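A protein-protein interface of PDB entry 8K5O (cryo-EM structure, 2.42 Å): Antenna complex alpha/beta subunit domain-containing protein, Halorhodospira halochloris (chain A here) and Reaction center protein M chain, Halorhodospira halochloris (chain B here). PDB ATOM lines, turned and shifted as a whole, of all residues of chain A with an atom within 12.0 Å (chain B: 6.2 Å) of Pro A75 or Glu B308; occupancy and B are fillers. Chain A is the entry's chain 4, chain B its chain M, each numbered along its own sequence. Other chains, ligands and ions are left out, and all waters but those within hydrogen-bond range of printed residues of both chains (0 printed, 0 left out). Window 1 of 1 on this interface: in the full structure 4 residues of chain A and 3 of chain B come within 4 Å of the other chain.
O of Phe A73 is in hydrogen-bond range of N of Glu B308 (2.8 Å).
O of Asp A72 touches CG of Glu B308, 3.5 Å away.
C of Tyr B307 touches O of Phe A73, 3.4 Å away.
CA of Leu A74 touches O of Ile B306, 3.3 Å away.
Pro A75 touches Ile B306.
CD of Pro A75 touches O of Tyr B307, at 3.2 Å.
CD of Pro A75 touches N of Glu B308, at 3.8 Å.
Asp A67 touches none of the printed residues of chain B.
Ser A68 touches none of the printed residues of chain B.
Printed residues of chain B within 4 Å of Asp A72: Glu B308.
Of the printed residues of chain B, Phe A73 touches Tyr B307 (3.4 Å) and Glu B308 (2.8 Å).
Of the printed residues of chain B, Leu A74 touches Ile B306.
Of the printed residues of chain B, Pro A75 touches Ile B306, Tyr B307 and Glu B308.
Of the printed residues of chain A, Tyr B307 touches Phe A73 and Pro A75.
Glu B308 touches three residues of chain A.
No residue of chain A comes within 4 Å of Glu B309.
No residue of chain A comes within 4 Å of Leu B310.
The nearest residue of chain A that does not touch Glu B308 is Leu A74 (4.8 Å).
Of the 10 printed residues of chain A, 4 touch a printed residue of chain B.
Printed residues of chain A that touch a printed residue of chain B: Asp A72, Phe A73, Leu A74 and Pro A75.
Printed residues of chain B that touch a printed residue of chain A: Ile B306, Tyr B307 and Glu B308.
Among the printed residues, 7 pairs touch across the chains.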
ATOM      1  N   ASP A  67     -13.883   8.282  -8.863  1.00  0.00           N
ATOM      2  CA  ASP A  67     -13.138   7.105  -9.279  1.00  0.00           C
ATOM      3  C   ASP A  67     -11.669   7.317  -8.945  1.00  0.00           C
ATOM      4  O   ASP A  67     -11.082   8.331  -9.332  1.00  0.00           O
ATOM      5  CB  ASP A  67     -13.317   6.848 -10.777  1.00  0.00           C
ATOM      6  CG  ASP A  67     -12.855   5.467 -11.194  1.00  0.00           C
ATOM      7  OD1 ASP A  67     -12.391   4.702 -10.324  1.00  0.00           O
ATOM      8  OD2 ASP A  67     -12.953   5.150 -12.398  1.00  0.00           O
ATOM      9  N   SER A  68     -11.086   6.370  -8.219  1.00  0.00           N
ATOM     10  CA  SER A  68      -9.691   6.487  -7.823  1.00  0.00           C
ATOM     11  C   SER A  68      -8.776   6.412  -9.038  1.00  0.00           C
ATOM     12  O   SER A  68      -9.102   5.793 -10.055  1.00  0.00           O
ATOM     13  CB  SER A  68      -9.329   5.390  -6.827  1.00  0.00           C
ATOM     14  OG  SER A  68      -9.405   4.114  -7.435  1.00  0.00           O
ATOM     15  N   PHE A  69      -7.617   7.063  -8.926  1.00  0.00           N
ATOM     16  CA  PHE A  69      -6.627   6.990  -9.993  1.00  0.00           C
ATOM     17  C   PHE A  69      -6.165   5.558 -10.207  1.00  0.00           C
ATOM     18  O   PHE A  69      -6.022   5.106 -11.349  1.00  0.00           O
ATOM     19  CB  PHE A  69      -5.438   7.896  -9.667  1.00  0.00           C
ATOM     20  CG  PHE A  69      -4.316   7.809 -10.657  1.00  0.00           C
ATOM     21  CD1 PHE A  69      -4.324   8.586 -11.800  1.00  0.00           C
ATOM     22  CD2 PHE A  69      -3.246   6.962 -10.436  1.00  0.00           C
ATOM     23  CE1 PHE A  69      -3.292   8.508 -12.710  1.00  0.00           C
ATOM     24  CE2 PHE A  69      -2.218   6.879 -11.342  1.00  0.00           C
ATOM     25  CZ  PHE A  69      -2.238   7.654 -12.478  1.00  0.00           C
ATOM     26  N   TYR A  70      -5.997   4.826  -9.130  1.00  0.00           N
ATOM     27  CA  TYR A  70      -5.559   3.488  -9.252  1.00  0.00           C
ATOM     28  C   TYR A  70      -6.708   2.579  -9.558  1.00  0.00           C
ATOM     29  O   TYR A  70      -7.750   2.695  -8.957  1.00  0.00           O
ATOM     30  CB  TYR A  70      -4.845   3.058  -7.976  1.00  0.00           C
ATOM     31  CG  TYR A  70      -3.688   3.901  -7.576  1.00  0.00           C
ATOM     32  CD1 TYR A  70      -2.630   4.118  -8.437  1.00  0.00           C
ATOM     33  CD2 TYR A  70      -3.647   4.466  -6.330  1.00  0.00           C
ATOM     34  CE1 TYR A  70      -1.562   4.886  -8.060  1.00  0.00           C
ATOM     35  CE2 TYR A  70      -2.592   5.243  -5.943  1.00  0.00           C
ATOM     36  CZ  TYR A  70      -1.556   5.445  -6.806  1.00  0.00           C
ATOM     37  OH  TYR A  70      -0.532   6.218  -6.383  1.00  0.00           O
ATOM     38  N   SER A  71      -6.525   1.642 -10.469  1.00  0.00           N
ATOM     39  CA  SER A  71      -7.543   0.664 -10.808  1.00  0.00           C
ATOM     40  C   SER A  71      -7.238  -0.669 -10.138  1.00  0.00           C
ATOM     41  O   SER A  71      -6.097  -0.969  -9.784  1.00  0.00           O
ATOM     42  CB  SER A  71      -7.643   0.481 -12.324  1.00  0.00           C
ATOM     43  OG  SER A  71      -6.477  -0.127 -12.845  1.00  0.00           O
ATOM     44  N   ASP A  72      -8.288  -1.469  -9.961  1.00  0.00           N
ATOM     45  CA  ASP A  72      -8.181  -2.789  -9.360  1.00  0.00           C
ATOM     46  C   ASP A  72      -8.054  -3.890 -10.404  1.00  0.00           C
ATOM     47  O   ASP A  72      -8.312  -5.058 -10.098  1.00  0.00           O
ATOM     48  CB  ASP A  72      -9.387  -3.055  -8.459  1.00  0.00           C
ATOM     49  CG  ASP A  72      -9.545  -2.015  -7.370  1.00  0.00           C
ATOM     50  OD1 ASP A  72      -8.745  -1.055  -7.338  1.00  0.00           O
ATOM     51  OD2 ASP A  72     -10.472  -2.155  -6.546  1.00  0.00           O
ATOM     52  N   PHE A  73      -7.668  -3.539 -11.633  1.00  0.00           N
ATOM     53  CA  PHE A  73      -7.594  -4.532 -12.698  1.00  0.00           C
ATOM     54  C   PHE A  73      -6.511  -5.566 -12.432  1.00  0.00           C
ATOM     55  O   PHE A  73      -6.672  -6.735 -12.796  1.00  0.00           O
ATOM     56  CB  PHE A  73      -7.348  -3.851 -14.042  1.00  0.00           C
ATOM     57  CG  PHE A  73      -7.370  -4.794 -15.209  1.00  0.00           C
ATOM     58  CD1 PHE A  73      -8.510  -5.523 -15.501  1.00  0.00           C
ATOM     59  CD2 PHE A  73      -6.251  -4.966 -16.004  1.00  0.00           C
ATOM     60  CE1 PHE A  73      -8.536  -6.397 -16.567  1.00  0.00           C
ATOM     61  CE2 PHE A  73      -6.275  -5.841 -17.071  1.00  0.00           C
ATOM     62  CZ  PHE A  73      -7.419  -6.553 -17.352  1.00  0.00           C
ATOM     63  N   LEU A  74      -5.407  -5.167 -11.803  1.00  0.00           N
ATOM     64  CA  LEU A  74      -4.291  -6.065 -11.509  1.00  0.00           C
ATOM     65  C   LEU A  74      -3.982  -6.024 -10.019  1.00  0.00           C
ATOM     66  O   LEU A  74      -3.071  -5.310  -9.578  1.00  0.00           O
ATOM     67  CB  LEU A  74      -3.065  -5.702 -12.346  1.00  0.00           C
ATOM     68  CG  LEU A  74      -3.295  -5.677 -13.856  1.00  0.00           C
ATOM     69  CD1 LEU A  74      -2.016  -5.332 -14.599  1.00  0.00           C
ATOM     70  CD2 LEU A  74      -3.843  -7.012 -14.310  1.00  0.00           C
ATOM     71  N   PRO A  75      -4.722  -6.791  -9.208  1.00  0.00           N
ATOM     72  CA  PRO A  75      -4.525  -6.822  -7.741  1.00  0.00           C
ATOM     73  C   PRO A  75      -3.219  -7.498  -7.343  1.00  0.00           C
ATOM     74  O   PRO A  75      -3.182  -8.593  -6.776  1.00  0.00           O
ATOM     75  CB  PRO A  75      -5.746  -7.614  -7.267  1.00  0.00           C
ATOM     76  CG  PRO A  75      -6.751  -7.435  -8.303  1.00  0.00           C
ATOM     77  CD  PRO A  75      -6.016  -7.375  -9.594  1.00  0.00           C
ATOM     78  N   THR A  76      -2.106  -6.839  -7.631  1.00  0.00           N
ATOM     79  CA  THR A  76      -0.802  -7.412  -7.328  1.00  0.00           C
ATOM     80  C   THR A  76      -0.177  -6.737  -6.115  1.00  0.00           C
ATOM     81  O   THR A  76      -0.871  -6.383  -5.163  1.00  0.00           O
ATOM     82  CB  THR A  76       0.157  -7.300  -8.524  1.00  0.00           C
ATOM     83  OG1 THR A  76       0.621  -5.952  -8.643  1.00  0.00           O
ATOM     84  CG2 THR A  76      -0.537  -7.708  -9.808  1.00  0.00           C
ATOM     85  N   ILE B 306      -1.757 -11.333 -11.546  1.00  0.00           N
ATOM     86  CA  ILE B 306      -2.999 -11.426 -10.790  1.00  0.00           C
ATOM     87  C   ILE B 306      -4.009 -10.518 -11.466  1.00  0.00           C
ATOM     88  O   ILE B 306      -3.751  -9.325 -11.667  1.00  0.00           O
ATOM     89  CB  ILE B 306      -2.818 -11.052  -9.311  1.00  0.00           C
ATOM     90  CG1 ILE B 306      -1.916 -12.064  -8.604  1.00  0.00           C
ATOM     91  CG2 ILE B 306      -4.162 -10.999  -8.619  1.00  0.00           C
ATOM     92  CD1 ILE B 306      -0.467 -11.718  -8.634  1.00  0.00           C
ATOM     93  N   TYR B 307      -5.152 -11.081 -11.821  1.00  0.00           N
ATOM     94  CA  TYR B 307      -6.161 -10.379 -12.592  1.00  0.00           C
ATOM     95  C   TYR B 307      -7.268  -9.863 -11.688  1.00  0.00           C
ATOM     96  O   TYR B 307      -7.319 -10.155 -10.492  1.00  0.00           O
ATOM     97  CB  TYR B 307      -6.725 -11.298 -13.674  1.00  0.00           C
ATOM     98  CG  TYR B 307      -5.665 -11.760 -14.632  1.00  0.00           C
ATOM     99  CD1 TYR B 307      -5.039 -10.858 -15.475  1.00  0.00           C
ATOM    100  CD2 TYR B 307      -5.277 -13.086 -14.683  1.00  0.00           C
ATOM    101  CE1 TYR B 307      -4.066 -11.263 -16.347  1.00  0.00           C
ATOM    102  CE2 TYR B 307      -4.301 -13.501 -15.553  1.00  0.00           C
ATOM    103  CZ  TYR B 307      -3.700 -12.583 -16.383  1.00  0.00           C
ATOM    104  OH  TYR B 307      -2.727 -12.983 -17.257  1.00  0.00           O
ATOM    105  N   GLU B 308      -8.159  -9.078 -12.288  1.00  0.00           N
ATOM    106  CA  GLU B 308      -9.288  -8.523 -11.562  1.00  0.00           C
ATOM    107  C   GLU B 308     -10.075  -9.640 -10.899  1.00  0.00           C
ATOM    108  O   GLU B 308     -10.370 -10.662 -11.525  1.00  0.00           O
ATOM    109  CB  GLU B 308     -10.183  -7.737 -12.520  1.00  0.00           C
ATOM    110  CG  GLU B 308     -10.932  -6.582 -11.892  1.00  0.00           C
ATOM    111  CD  GLU B 308     -11.544  -5.663 -12.928  1.00  0.00           C
ATOM    112  OE1 GLU B 308     -11.969  -6.165 -13.990  1.00  0.00           O
ATOM    113  OE2 GLU B 308     -11.603  -4.438 -12.684  1.00  0.00           O
ATOM    114  N   GLU B 309     -10.389  -9.458  -9.619  1.00  0.00           N
ATOM    115  CA  GLU B 309     -11.206 -10.434  -8.915  1.00  0.00           C
ATOM    116  C   GLU B 309     -12.559 -10.548  -9.599  1.00  0.00           C
ATOM    117  O   GLU B 309     -13.188  -9.537  -9.926  1.00  0.00           O
ATOM    118  CB  GLU B 309     -11.366 -10.036  -7.447  1.00  0.00           C
ATOM    119  CG  GLU B 309     -12.024  -8.686  -7.221  1.00  0.00           C
ATOM    120  CD  GLU B 309     -12.117  -8.314  -5.754  1.00  0.00           C
ATOM    121  OE1 GLU B 309     -11.666  -9.110  -4.906  1.00  0.00           O
ATOM    122  OE2 GLU B 309     -12.639  -7.221  -5.450  1.00  0.00           O
ATOM    123  N   LEU B 310     -12.990 -11.778  -9.851  1.00  0.00           N
ATOM    124  CA  LEU B 310     -14.250 -11.985 -10.547  1.00  0.00           C
ATOM    125  C   LEU B 310     -15.424 -11.626  -9.651  1.00  0.00           C
ATOM    126  O   LEU B 310     -15.390 -11.838  -8.437  1.00  0.00           O
ATOM    127  CB  LEU B 310     -14.380 -13.433 -11.012  1.00  0.00           C
ATOM    128  CG  LEU B 310     -13.297 -13.974 -11.941  1.00  0.00           C
ATOM    129  CD1 LEU B 310     -13.339 -15.486 -11.950  1.00  0.00           C
ATOM    130  CD2 LEU B 310     -13.468 -13.421 -13.344  1.00  0.00           C
